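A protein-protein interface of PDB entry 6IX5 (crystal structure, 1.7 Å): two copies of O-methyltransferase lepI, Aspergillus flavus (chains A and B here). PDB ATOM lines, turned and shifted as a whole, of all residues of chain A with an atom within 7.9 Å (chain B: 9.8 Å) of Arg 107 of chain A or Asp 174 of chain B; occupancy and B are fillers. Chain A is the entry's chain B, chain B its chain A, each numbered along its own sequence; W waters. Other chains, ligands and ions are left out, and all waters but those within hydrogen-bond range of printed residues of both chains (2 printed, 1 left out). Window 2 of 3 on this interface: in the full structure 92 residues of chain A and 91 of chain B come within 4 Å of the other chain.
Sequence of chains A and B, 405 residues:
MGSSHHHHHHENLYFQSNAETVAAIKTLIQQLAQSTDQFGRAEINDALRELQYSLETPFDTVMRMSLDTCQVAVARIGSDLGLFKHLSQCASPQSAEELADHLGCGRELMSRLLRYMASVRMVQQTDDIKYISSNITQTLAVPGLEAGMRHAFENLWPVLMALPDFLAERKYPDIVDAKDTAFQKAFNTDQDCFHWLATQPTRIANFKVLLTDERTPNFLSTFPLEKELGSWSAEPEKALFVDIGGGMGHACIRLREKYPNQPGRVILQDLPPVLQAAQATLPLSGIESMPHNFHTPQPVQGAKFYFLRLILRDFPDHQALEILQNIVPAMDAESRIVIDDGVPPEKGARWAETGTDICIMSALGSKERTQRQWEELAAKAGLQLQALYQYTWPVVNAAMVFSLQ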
ATOM      1  N   SER A  95      31.450 -25.422  21.143  1.00  0.00           N
ATOM      2  CA  SER A  95      30.627 -26.204  20.228  1.00  0.00           C
ATOM      3  C   SER A  95      30.206 -25.361  19.015  1.00  0.00           C
ATOM      4  O   SER A  95      30.220 -24.127  19.059  1.00  0.00           O
ATOM      5  CB  SER A  95      29.376 -26.721  20.961  1.00  0.00           C
ATOM      6  OG  SER A  95      28.537 -25.618  21.238  1.00  0.00           O
ATOM      7  N   ALA A  96      29.805 -26.042  17.918  1.00  0.00           N
ATOM      8  CA  ALA A  96      29.277 -25.298  16.767  1.00  0.00           C
ATOM      9  C   ALA A  96      28.083 -24.452  17.170  1.00  0.00           C
ATOM     10  O   ALA A  96      27.902 -23.337  16.672  1.00  0.00           O
ATOM     11  CB  ALA A  96      28.874 -26.249  15.631  1.00  0.00           C
ATOM     12  N   GLU A  97      27.234 -24.987  18.074  1.00  0.00           N
ATOM     13  CA  GLU A  97      26.062 -24.258  18.512  1.00  0.00           C
ATOM     14  C   GLU A  97      26.464 -22.960  19.210  1.00  0.00           C
ATOM     15  O   GLU A  97      25.876 -21.901  18.962  1.00  0.00           O
ATOM     16  CB  GLU A  97      25.237 -25.190  19.433  1.00  0.00           C
ATOM     17  CG  GLU A  97      24.169 -24.571  20.259  1.00  0.00           C
ATOM     18  CD  GLU A  97      23.369 -25.615  21.087  1.00  0.00           C
ATOM     19  OE1 GLU A  97      22.307 -25.242  21.610  1.00  0.00           O
ATOM     20  OE2 GLU A  97      23.789 -26.794  21.232  1.00  0.00           O
ATOM     21  N   GLU A  98      27.456 -23.033  20.101  1.00  0.00           N
ATOM     22  CA  GLU A  98      27.898 -21.848  20.828  1.00  0.00           C
ATOM     23  C   GLU A  98      28.477 -20.822  19.877  1.00  0.00           C
ATOM     24  O   GLU A  98      28.214 -19.619  20.009  1.00  0.00           O
ATOM     25  CB  GLU A  98      28.934 -22.240  21.872  1.00  0.00           C
ATOM     26  CG  GLU A  98      28.326 -22.932  23.114  1.00  0.00           C
ATOM     27  CD  GLU A  98      29.385 -23.609  24.023  1.00  0.00           C
ATOM     28  OE1 GLU A  98      30.456 -24.102  23.550  1.00  0.00           O
ATOM     29  OE2 GLU A  98      29.126 -23.704  25.234  1.00  0.00           O
ATOM     30  N   LEU A  99      29.295 -21.281  18.937  1.00  0.00           N
ATOM     31  CA  LEU A  99      29.868 -20.365  17.957  1.00  0.00           C
ATOM     32  C   LEU A  99      28.779 -19.733  17.105  1.00  0.00           C
ATOM     33  O   LEU A  99      28.795 -18.517  16.870  1.00  0.00           O
ATOM     34  CB  LEU A  99      30.896 -21.105  17.084  1.00  0.00           C
ATOM     35  CG  LEU A  99      32.161 -21.462  17.895  1.00  0.00           C
ATOM     36  CD1 LEU A  99      33.007 -22.528  17.177  1.00  0.00           C
ATOM     37  CD2 LEU A  99      33.028 -20.217  18.260  1.00  0.00           C
ATOM     38  N   ALA A 100      27.817 -20.536  16.653  1.00  0.00           N
ATOM     39  CA  ALA A 100      26.749 -20.010  15.795  1.00  0.00           C
ATOM     40  C   ALA A 100      25.967 -18.912  16.517  1.00  0.00           C
ATOM     41  O   ALA A 100      25.733 -17.823  15.976  1.00  0.00           O
ATOM     42  CB  ALA A 100      25.819 -21.163  15.366  1.00  0.00           C
ATOM     43  N   ASP A 101      25.616 -19.164  17.773  1.00  0.00           N
ATOM     44  CA  ASP A 101      24.800 -18.210  18.522  1.00  0.00           C
ATOM     45  C   ASP A 101      25.571 -16.942  18.836  1.00  0.00           C
ATOM     46  O   ASP A 101      25.015 -15.839  18.764  1.00  0.00           O
ATOM     47  CB  ASP A 101      24.322 -18.862  19.805  1.00  0.00           C
ATOM     48  CG  ASP A 101      23.333 -19.971  19.548  1.00  0.00           C
ATOM     49  OD1 ASP A 101      22.975 -20.218  18.351  1.00  0.00           O
ATOM     50  OD2 ASP A 101      22.929 -20.611  20.548  1.00  0.00           O
ATOM     51  N   GLY A 104      26.140 -15.012  15.311  1.00  0.00           N
ATOM     52  CA  GLY A 104      24.983 -14.697  14.461  1.00  0.00           C
ATOM     53  C   GLY A 104      24.967 -15.464  13.145  1.00  0.00           C
ATOM     54  O   GLY A 104      24.739 -14.882  12.081  1.00  0.00           O
ATOM     55  N   CYS A 105      25.202 -16.774  13.212  1.00  0.00           N
ATOM     56  CA  CYS A 105      25.198 -17.655  12.058  1.00  0.00           C
ATOM     57  C   CYS A 105      24.188 -18.763  12.280  1.00  0.00           C
ATOM     58  O   CYS A 105      24.004 -19.220  13.419  1.00  0.00           O
ATOM     59  CB  CYS A 105      26.604 -18.249  11.861  1.00  0.00           C
ATOM     60  SG  CYS A 105      26.832 -19.238  10.374  1.00  0.00           S
ATOM     61  N   GLY A 106      23.489 -19.151  11.197  1.00  0.00           N
ATOM     62  CA  GLY A 106      22.626 -20.311  11.240  1.00  0.00           C
ATOM     63  C   GLY A 106      23.382 -21.496  11.820  1.00  0.00           C
ATOM     64  O   GLY A 106      24.564 -21.683  11.541  1.00  0.00           O
ATOM     65  N   ARG A 107      22.725 -22.296  12.660  1.00  0.00           N
ATOM     66  CA  ARG A 107      23.456 -23.354  13.363  1.00  0.00           C
ATOM     67  C   ARG A 107      23.939 -24.458  12.440  1.00  0.00           C
ATOM     68  O   ARG A 107      25.035 -24.993  12.647  1.00  0.00           O
ATOM     69  CB  ARG A 107      22.582 -23.949  14.456  1.00  0.00           C
ATOM     70  CG  ARG A 107      22.595 -23.100  15.704  1.00  0.00           C
ATOM     71  CD  ARG A 107      21.525 -23.550  16.661  1.00  0.00           C
ATOM     72  NE  ARG A 107      21.706 -22.997  18.007  1.00  0.00           N
ATOM     73  CZ  ARG A 107      21.150 -23.544  19.093  1.00  0.00           C
ATOM     74  NH1 ARG A 107      20.403 -24.641  18.963  1.00  0.00           N
ATOM     75  NH2 ARG A 107      21.347 -23.006  20.298  1.00  0.00           N
ATOM     76  N   GLU A 108      23.108 -24.899  11.484  1.00  0.00           N
ATOM     77  CA  GLU A 108      23.568 -25.941  10.569  1.00  0.00           C
ATOM     78  C   GLU A 108      24.666 -25.410   9.643  1.00  0.00           C
ATOM     79  O   GLU A 108      25.653 -26.104   9.369  1.00  0.00           O
ATOM     80  CB  GLU A 108      22.400 -26.495   9.764  1.00  0.00           C
ATOM     81  CG  GLU A 108      22.791 -27.663   8.859  1.00  0.00           C
ATOM     82  CD  GLU A 108      23.412 -28.838   9.610  1.00  0.00           C
ATOM     83  OE1 GLU A 108      24.034 -29.704   8.936  1.00  0.00           O
ATOM     84  OE2 GLU A 108      23.279 -28.899  10.864  1.00  0.00           O
ATOM     85  N   LEU A 109      24.513 -24.178   9.170  1.00  0.00           N
ATOM     86  CA  LEU A 109      25.554 -23.557   8.347  1.00  0.00           C
ATOM     87  C   LEU A 109      26.884 -23.504   9.100  1.00  0.00           C
ATOM     88  O   LEU A 109      27.944 -23.864   8.561  1.00  0.00           O
ATOM     89  CB  LEU A 109      25.125 -22.142   7.934  1.00  0.00           C
ATOM     90  CG  LEU A 109      26.170 -21.286   7.182  1.00  0.00           C
ATOM     91  CD1 LEU A 109      26.607 -21.974   5.913  1.00  0.00           C
ATOM     92  CD2 LEU A 109      25.603 -19.884   6.860  1.00  0.00           C
ATOM     93  N   MET A 110      26.840 -23.056  10.356  1.00  0.00           N
ATOM     94  CA  MET A 110      28.058 -22.944  11.145  1.00  0.00           C
ATOM     95  C   MET A 110      28.699 -24.311  11.330  1.00  0.00           C
ATOM     96  O   MET A 110      29.934 -24.466  11.238  1.00  0.00           O
ATOM     97  CB  MET A 110      27.731 -22.322  12.511  1.00  0.00           C
ATOM     98  CG  MET A 110      28.927 -22.255  13.413  1.00  0.00           C
ATOM     99  SD  MET A 110      30.247 -21.139  12.849  1.00  0.00           S
ATOM    100  CE  MET A 110      29.611 -19.643  13.346  1.00  0.00           C
ATOM    101  N   SER A 111      27.877 -25.323  11.598  1.00  0.00           N
ATOM    102  CA  SER A 111      28.445 -26.639  11.823  1.00  0.00           C
ATOM    103  C   SER A 111      29.135 -27.155  10.561  1.00  0.00           C
ATOM    104  O   SER A 111      30.237 -27.723  10.633  1.00  0.00           O
ATOM    105  CB  SER A 111      27.350 -27.592  12.273  1.00  0.00           C
ATOM    106  OG  SER A 111      27.909 -28.873  12.341  1.00  0.00           O
ATOM    107  N   ARG A 112      28.509 -26.947   9.396  1.00  0.00           N
ATOM    108  CA  ARG A 112      29.116 -27.404   8.140  1.00  0.00           C
ATOM    109  C   ARG A 112      30.369 -26.613   7.801  1.00  0.00           C
ATOM    110  O   ARG A 112      31.361 -27.188   7.304  1.00  0.00           O
ATOM    111  CB  ARG A 112      28.104 -27.304   6.998  1.00  0.00           C
ATOM    112  CG  ARG A 112      26.903 -28.274   7.227  1.00  0.00           C
ATOM    113  CD  ARG A 112      25.773 -27.945   6.294  1.00  0.00           C
ATOM    114  NE  ARG A 112      26.062 -28.419   4.953  1.00  0.00           N
ATOM    115  CZ  ARG A 112      25.192 -28.360   3.955  1.00  0.00           C
ATOM    116  NH1 ARG A 112      23.966 -27.807   4.138  1.00  0.00           N
ATOM    117  NH2 ARG A 112      25.538 -28.858   2.781  1.00  0.00           N
ATOM    118  N   LEU A 113      30.356 -25.294   8.053  1.00  0.00           N
ATOM    119  CA  LEU A 113      31.556 -24.505   7.808  1.00  0.00           C
ATOM    120  C   LEU A 113      32.707 -24.977   8.703  1.00  0.00           C
ATOM    121  O   LEU A 113      33.868 -25.061   8.247  1.00  0.00           O
ATOM    122  CB  LEU A 113      31.293 -23.017   8.049  1.00  0.00           C
ATOM    123  CG  LEU A 113      30.323 -22.345   7.068  1.00  0.00           C
ATOM    124  CD1 LEU A 113      29.918 -20.939   7.550  1.00  0.00           C
ATOM    125  CD2 LEU A 113      31.005 -22.235   5.751  1.00  0.00           C
ATOM    126  N   LEU A 114      32.414 -25.224   9.992  1.00  0.00           N
ATOM    127  CA  LEU A 114      33.462 -25.665  10.913  1.00  0.00           C
ATOM    128  C   LEU A 114      34.015 -27.023  10.531  1.00  0.00           C
ATOM    129  O   LEU A 114      35.223 -27.262  10.663  1.00  0.00           O
ATOM    130  CB  LEU A 114      32.948 -25.702  12.367  1.00  0.00           C
ATOM    131  CG  LEU A 114      32.712 -24.301  12.936  1.00  0.00           C
ATOM    132  CD1 LEU A 114      31.852 -24.433  14.236  1.00  0.00           C
ATOM    133  CD2 LEU A 114      34.018 -23.535  13.294  1.00  0.00           C
ATOM    134  N   LEU B 163      29.262 -17.022  -2.725  1.00  0.00           N
ATOM    135  CA  LEU B 163      28.741 -17.503  -1.444  1.00  0.00           C
ATOM    136  C   LEU B 163      28.941 -16.513  -0.297  1.00  0.00           C
ATOM    137  O   LEU B 163      27.978 -16.293   0.477  1.00  0.00           O
ATOM    138  CB  LEU B 163      29.342 -18.887  -1.115  1.00  0.00           C
ATOM    139  CG  LEU B 163      28.885 -19.523   0.220  1.00  0.00           C
ATOM    140  CD1 LEU B 163      27.417 -19.937   0.094  1.00  0.00           C
ATOM    141  CD2 LEU B 163      29.782 -20.729   0.597  1.00  0.00           C
ATOM    142  N   PHE B 166      26.479 -13.637  -0.597  1.00  0.00           N
ATOM    143  CA  PHE B 166      25.145 -14.207  -0.440  1.00  0.00           C
ATOM    144  C   PHE B 166      24.804 -14.399   1.032  1.00  0.00           C
ATOM    145  O   PHE B 166      23.753 -13.936   1.507  1.00  0.00           O
ATOM    146  CB  PHE B 166      25.042 -15.542  -1.194  1.00  0.00           C
ATOM    147  CG  PHE B 166      23.753 -16.268  -0.936  1.00  0.00           C
ATOM    148  CD1 PHE B 166      22.561 -15.795  -1.483  1.00  0.00           C
ATOM    149  CD2 PHE B 166      23.720 -17.387  -0.117  1.00  0.00           C
ATOM    150  CE1 PHE B 166      21.356 -16.451  -1.243  1.00  0.00           C
ATOM    151  CE2 PHE B 166      22.510 -18.045   0.130  1.00  0.00           C
ATOM    152  CZ  PHE B 166      21.320 -17.554  -0.442  1.00  0.00           C
ATOM    153  N   LEU B 167      25.690 -15.075   1.774  1.00  0.00           N
ATOM    154  CA  LEU B 167      25.446 -15.327   3.195  1.00  0.00           C
ATOM    155  C   LEU B 167      25.384 -14.032   3.995  1.00  0.00           C
ATOM    156  O   LEU B 167      24.563 -13.903   4.921  1.00  0.00           O
ATOM    157  CB  LEU B 167      26.535 -16.247   3.758  1.00  0.00           C
ATOM    158  CG  LEU B 167      26.586 -17.681   3.153  1.00  0.00           C
ATOM    159  CD1 LEU B 167      27.776 -18.484   3.696  1.00  0.00           C
ATOM    160  CD2 LEU B 167      25.295 -18.502   3.398  1.00  0.00           C
ATOM    161  N   ARG B 170      22.096 -12.175   3.514  1.00  0.00           N
ATOM    162  CA  ARG B 170      20.953 -12.906   4.042  1.00  0.00           C
ATOM    163  C   ARG B 170      21.094 -13.240   5.521  1.00  0.00           C
ATOM    164  O   ARG B 170      20.260 -13.974   6.058  1.00  0.00           O
ATOM    165  CB  ARG B 170      20.739 -14.190   3.228  1.00  0.00           C
ATOM    166  CG  ARG B 170      20.250 -13.877   1.802  1.00  0.00           C
ATOM    167  CD  ARG B 170      18.778 -13.449   1.835  1.00  0.00           C
ATOM    168  NE  ARG B 170      18.042 -14.594   2.353  1.00  0.00           N
ATOM    169  CZ  ARG B 170      17.703 -15.647   1.608  1.00  0.00           C
ATOM    170  NH1 ARG B 170      17.976 -15.667   0.289  1.00  0.00           N
ATOM    171  NH2 ARG B 170      17.073 -16.673   2.182  1.00  0.00           N
ATOM    172  N   LYS B 171      22.138 -12.739   6.176  1.00  0.00           N
ATOM    173  CA  LYS B 171      22.369 -12.935   7.605  1.00  0.00           C
ATOM    174  C   LYS B 171      22.507 -14.421   7.933  1.00  0.00           C
ATOM    175  O   LYS B 171      21.966 -14.920   8.923  1.00  0.00           O
ATOM    176  CB  LYS B 171      21.276 -12.246   8.446  1.00  0.00           C
ATOM    177  CG  LYS B 171      21.207 -10.748   8.146  1.00  0.00           C
ATOM    178  CD  LYS B 171      19.856 -10.151   8.563  1.00  0.00           C
ATOM    179  CE  LYS B 171      19.856  -9.588   9.992  1.00  0.00           C
ATOM    180  NZ  LYS B 171      18.451  -9.548  10.571  1.00  0.00           N
ATOM    181  N   TYR B 172      23.283 -15.131   7.087  1.00  0.00           N
ATOM    182  CA  TYR B 172      23.790 -16.464   7.398  1.00  0.00           C
ATOM    183  C   TYR B 172      22.676 -17.469   7.650  1.00  0.00           C
ATOM    184  O   TYR B 172      22.609 -18.073   8.745  1.00  0.00           O
ATOM    185  CB  TYR B 172      24.757 -16.362   8.587  1.00  0.00           C
ATOM    186  CG  TYR B 172      25.902 -15.448   8.194  1.00  0.00           C
ATOM    187  CD1 TYR B 172      26.964 -15.928   7.394  1.00  0.00           C
ATOM    188  CD2 TYR B 172      25.882 -14.100   8.519  1.00  0.00           C
ATOM    189  CE1 TYR B 172      27.951 -15.089   6.961  1.00  0.00           C
ATOM    190  CE2 TYR B 172      26.892 -13.244   8.103  1.00  0.00           C
ATOM    191  CZ  TYR B 172      27.917 -13.734   7.321  1.00  0.00           C
ATOM    192  OH  TYR B 172      28.894 -12.866   6.885  1.00  0.00           O
ATOM    193  N   PRO B 173      21.795 -17.678   6.668  1.00  0.00           N
ATOM    194  CA  PRO B 173      20.730 -18.673   6.823  1.00  0.00           C
ATOM    195  C   PRO B 173      21.267 -20.076   6.630  1.00  0.00           C
ATOM    196  O   PRO B 173      22.262 -20.292   5.936  1.00  0.00           O
ATOM    197  CB  PRO B 173      19.760 -18.316   5.689  1.00  0.00           C
ATOM    198  CG  PRO B 173      20.732 -17.856   4.579  1.00  0.00           C
ATOM    199  CD  PRO B 173      21.781 -17.067   5.328  1.00  0.00           C
ATOM    200  N   ASP B 174      20.615 -21.032   7.277  1.00  0.00           N
ATOM    201  CA  ASP B 174      20.812 -22.427   6.885  1.00  0.00           C
ATOM    202  C   ASP B 174      20.276 -22.591   5.465  1.00  0.00           C
ATOM    203  O   ASP B 174      19.126 -22.239   5.193  1.00  0.00           O
ATOM    204  CB  ASP B 174      20.095 -23.358   7.853  1.00  0.00           C
ATOM    205  CG  ASP B 174      20.702 -23.315   9.256  1.00  0.00           C
ATOM    206  OD1 ASP B 174      21.875 -22.931   9.385  1.00  0.00           O
ATOM    207  OD2 ASP B 174      20.024 -23.652  10.245  1.00  0.00           O
ATOM    208  N   ILE B 175      21.097 -23.093   4.551  1.00  0.00           N
ATOM    209  CA  ILE B 175      20.645 -23.291   3.173  1.00  0.00           C
ATOM    210  C   ILE B 175      19.944 -24.633   3.066  1.00  0.00           C
ATOM    211  O   ILE B 175      20.510 -25.671   3.432  1.00  0.00           O
ATOM    212  CB  ILE B 175      21.808 -23.201   2.189  1.00  0.00           C
ATOM    213  CG1 ILE B 175      22.321 -21.755   2.172  1.00  0.00           C
ATOM    214  CG2 ILE B 175      21.381 -23.721   0.810  1.00  0.00           C
ATOM    215  CD1 ILE B 175      23.667 -21.624   1.560  1.00  0.00           C
ATOM    216  N   VAL B 176      18.705 -24.616   2.577  1.00  0.00           N
ATOM    217  CA  VAL B 176      17.849 -25.793   2.651  1.00  0.00           C
ATOM    218  C   VAL B 176      17.187 -26.091   1.315  1.00  0.00           C
ATOM    219  O   VAL B 176      16.584 -27.165   1.152  1.00  0.00           O
ATOM    220  CB  VAL B 176      16.776 -25.623   3.759  1.00  0.00           C
ATOM    221  CG1 VAL B 176      17.432 -25.502   5.138  1.00  0.00           C
ATOM    222  CG2 VAL B 176      15.872 -24.403   3.490  1.00  0.00           C
ATOM    223  N   ASP B 177      17.243 -25.144   0.369  1.00  0.00           N
ATOM    224  CA  ASP B 177      16.389 -25.152  -0.825  1.00  0.00           C
ATOM    225  C   ASP B 177      17.246 -24.936  -2.066  1.00  0.00           C
ATOM    226  O   ASP B 177      18.020 -23.979  -2.114  1.00  0.00           O
ATOM    227  CB  ASP B 177      15.324 -24.037  -0.697  1.00  0.00           C
ATOM    228  CG  ASP B 177      14.398 -23.878  -1.944  1.00  0.00           C
ATOM    229  OD1 ASP B 177      14.443 -24.667  -2.909  1.00  0.00           O
ATOM    230  OD2 ASP B 177      13.594 -22.896  -1.930  1.00  0.00           O
ATOM    231  N   ALA B 178      17.097 -25.811  -3.071  1.00  0.00           N
ATOM    232  CA  ALA B 178      17.841 -25.658  -4.331  1.00  0.00           C
ATOM    233  C   ALA B 178      17.498 -24.352  -5.034  1.00  0.00           C
ATOM    234  O   ALA B 178      18.316 -23.833  -5.804  1.00  0.00           O
ATOM    235  CB  ALA B 178      17.574 -26.840  -5.276  1.00  0.00           C
ATOM    236  N   ASP B 180      17.137 -21.469  -3.467  1.00  0.00           N
ATOM    237  CA  ASP B 180      17.534 -20.309  -2.654  1.00  0.00           C
ATOM    238  C   ASP B 180      18.917 -20.551  -2.086  1.00  0.00           C
ATOM    239  O   ASP B 180      19.076 -20.832  -0.899  1.00  0.00           O
ATOM    240  CB  ASP B 180      16.533 -20.051  -1.519  1.00  0.00           C
ATOM    241  CG  ASP B 180      16.808 -18.750  -0.773  1.00  0.00           C
ATOM    242  OD1 ASP B 180      17.627 -17.925  -1.257  1.00  0.00           O
ATOM    243  OD2 ASP B 180      16.180 -18.547   0.303  1.00  0.00           O
ATOM    244  N   THR B 181      19.925 -20.495  -2.943  1.00  0.00           N
ATOM    245  CA  THR B 181      21.284 -20.690  -2.491  1.00  0.00           C
ATOM    246  C   THR B 181      22.172 -19.741  -3.292  1.00  0.00           C
ATOM    247  O   THR B 181      21.691 -18.773  -3.917  1.00  0.00           O
ATOM    248  CB  THR B 181      21.663 -22.182  -2.574  1.00  0.00           C
ATOM    249  OG1 THR B 181      22.980 -22.347  -2.042  1.00  0.00           O
ATOM    250  CG2 THR B 181      21.567 -22.728  -4.004  1.00  0.00           C
ATOM    251  N   ALA B 182      23.483 -19.988  -3.265  1.00  0.00           N
ATOM    252  CA  ALA B 182      24.380 -19.020  -3.897  1.00  0.00           C
ATOM    253  C   ALA B 182      24.276 -19.065  -5.417  1.00  0.00           C
ATOM    254  O   ALA B 182      24.608 -18.079  -6.070  1.00  0.00           O
ATOM    255  CB  ALA B 182      25.841 -19.256  -3.479  1.00  0.00           C
ATOM    256  N   MET B 361      26.190 -27.572  -1.355  1.00  0.00           N
ATOM    257  CA  MET B 361      25.327 -26.630  -0.652  1.00  0.00           C
ATOM    258  C   MET B 361      25.136 -25.367  -1.477  1.00  0.00           C
ATOM    259  O   MET B 361      24.010 -24.857  -1.632  1.00  0.00           O
ATOM    260  CB  MET B 361      25.931 -26.268   0.721  1.00  0.00           C
ATOM    261  CG  MET B 361      25.058 -25.339   1.574  1.00  0.00           C
ATOM    262  SD  MET B 361      25.944 -24.800   3.057  1.00  0.00           S
ATOM    263  CE  MET B 361      27.195 -23.635   2.391  1.00  0.00           C
ATOM    264  N   GLY B 365      21.931 -26.615  -3.078  1.00  0.00           N
ATOM    265  CA  GLY B 365      21.157 -26.651  -1.857  1.00  0.00           C
ATOM    266  C   GLY B 365      21.181 -27.965  -1.092  1.00  0.00           C
ATOM    267  O   GLY B 365      20.444 -28.111  -0.091  1.00  0.00           O
ATOM    268  N   SER B 366      22.014 -28.916  -1.503  1.00  0.00           N
ATOM    269  CA  SER B 366      22.004 -30.265  -0.943  1.00  0.00           C
ATOM    270  C   SER B 366      23.169 -30.404   0.041  1.00  0.00           C
ATOM    271  O   SER B 366      23.652 -29.399   0.596  1.00  0.00           O
ATOM    272  CB  SER B 366      22.056 -31.310  -2.075  1.00  0.00           C
ATOM    273  OG  SER B 366      23.264 -31.182  -2.825  1.00  0.00           O
ATOM    274  N   LYS B 367      23.623 -31.635   0.284  1.00  0.00           N
ATOM    275  CA  LYS B 367      24.531 -31.862   1.410  1.00  0.00           C
ATOM    276  C   LYS B 367      25.060 -33.284   1.333  1.00  0.00           C
ATOM    277  O   LYS B 367      24.397 -34.167   0.786  1.00  0.00           O
ATOM    278  CB  LYS B 367      23.815 -31.630   2.768  1.00  0.00           C
ATOM    279  CG  LYS B 367      22.813 -32.722   3.057  1.00  0.00           C
ATOM    280  CD  LYS B 367      21.954 -32.463   4.326  1.00  0.00           C
ATOM    281  CE  LYS B 367      22.814 -32.054   5.524  1.00  0.00           C
ATOM    282  NZ  LYS B 367      23.471 -33.241   6.176  1.00  0.00           N
HETATM  283  O   HOH W   1      21.528 -15.943  12.184  1.00  0.00           O
HETATM  284  O   HOH W   2      24.666 -31.864   8.102  1.00  0.00           O
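No position is printed for both chains. Of the 14 pairs that touch across the chains among the printed residues, none has its exchanged pair printed and touching as well.
Among the printed residues, merely in contact across the chains: Gly 106 of chain A with Asp 174 of chain B (3.2 Å), Arg 112 of chain A with Lys 367 of chain B (3.3 Å), Leu 109 of chain A with Pro 173 of chain B (3.5 Å), Cys 105 of chain A with Tyr 172 of chain B (3.7 Å), Leu 109 of chain A with Leu 167 of chain B (3.7 Å), Gly 104 of chain A with Tyr 172 of chain B (3.8 Å), Leu 109 of chain A with Tyr 172 of chain B (3.9 Å) and Leu 109 of chain A with Met 361 of chain B (3.9 Å).
The side-chain carboxylate of Asp 174 of chain B sits at hydrogen-bond distance from the backbone NH of Glu 108 of chain A, at 3.1 Å. The backbone NH (N) of Gly 106 of chain A sits at hydrogen-bond distance from the backbone carbonyl oxygen (O) of Tyr 172 of chain B (2.8 Å). NH1 of Arg 112 of chain A lies close to SD of Met 361 of chain B (3.8 Å). The backbone carbonyl oxygen (O) of Ser 366 of chain B is in hydrogen-bond range of the guanidinium group (NH2) of Arg 112 of chain A, 2.9 Å away. The side-chain carboxylate (OD1) of Asp 174 of chain B is in hydrogen-bond range of the backbone NH (N) of Leu 109 of chain A, at 2.9 Å. The side-chain carboxylate (OD1) of Asp 174 of chain B sits at hydrogen-bond distance from the backbone NH (N) of Arg 107 of chain A (3.4 Å).
Hydrophobic or aromatic side chains of chain A within 4 Å of the printed part of chain B: Leu 109. Along chain A the printed residues that touch a printed residue of chain B span positions 104 to 112. Printed residues of chain B that touch a printed residue of chain A: Leu 167, Tyr 172, Pro 173, Asp 174, Met 361, Ser 366 and Lys 367. Hydrophobic or aromatic side chains of chain B that line the printed part of chain A: Leu 167, Tyr 172 and Met 361. Among the printed residues, 14 pairs touch across the chains.
OD2 of Asp 101 of chain A lies within salt-bridge range of NH2 of Arg 107 of chain A, at 2.9 Å. The backbone NH (N) of Tyr 172 of chain B sits at hydrogen-bond distance from the backbone carbonyl oxygen (O) of Leu 167 of chain B (2.8 Å). The backbone carbonyl oxygen (O) of Ala 100 of chain A lies within hydrogen-bond range of the backbone NH (N) of Cys 105 of chain A (3.0 Å). The side-chain carboxylate (OE1) of Glu 97 of chain A lies within salt-bridge range of the guanidinium group (NH2) of Arg 107 of chain A, 2.8 Å away. The side-chain hydroxyl (OG1) of Thr 181 of chain B is in hydrogen-bond range of the backbone carbonyl oxygen (O) of Met 361 of chain B.
Water W2 bridges the side-chain carboxylate (OE1) of Glu 108 of chain A (2.4 Å) and the side-chain amino group (NZ) of Lys 367 of chain B (2.7 Å). Water W1 bridges the backbone carbonyl oxygen of Gly 104 of chain A (3.4 Å) and the backbone carbonyl oxygen of Lys 171 of chain B (3.4 Å).
Arg 107 of chain A touches just one residue of chain B: Asp 174 (3.4 Å). Asp 174 of chain B touches four residues of chain A. No residue of chain B comes within 4 Å of Glu 97 of chain A. Printed residues of chain B within 4 Å of Gly 106 of chain A: Tyr 172 and Asp 174. Of the printed residues of chain B, Cys 105 of chain A touches Tyr 172. Of the printed residues of chain B, Glu 108 of chain A touches Asp 174 (3.1 Å). Ser 111 of chain A touches none of the printed residues of chain B. The nearest residue of chain B that does not touch Arg 107 of chain A is Tyr 172 of chain B (5.8 Å). The nearest residue of chain A that does not touch Asp 174 of chain B is Met 110 of chain A (5.1 Å).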
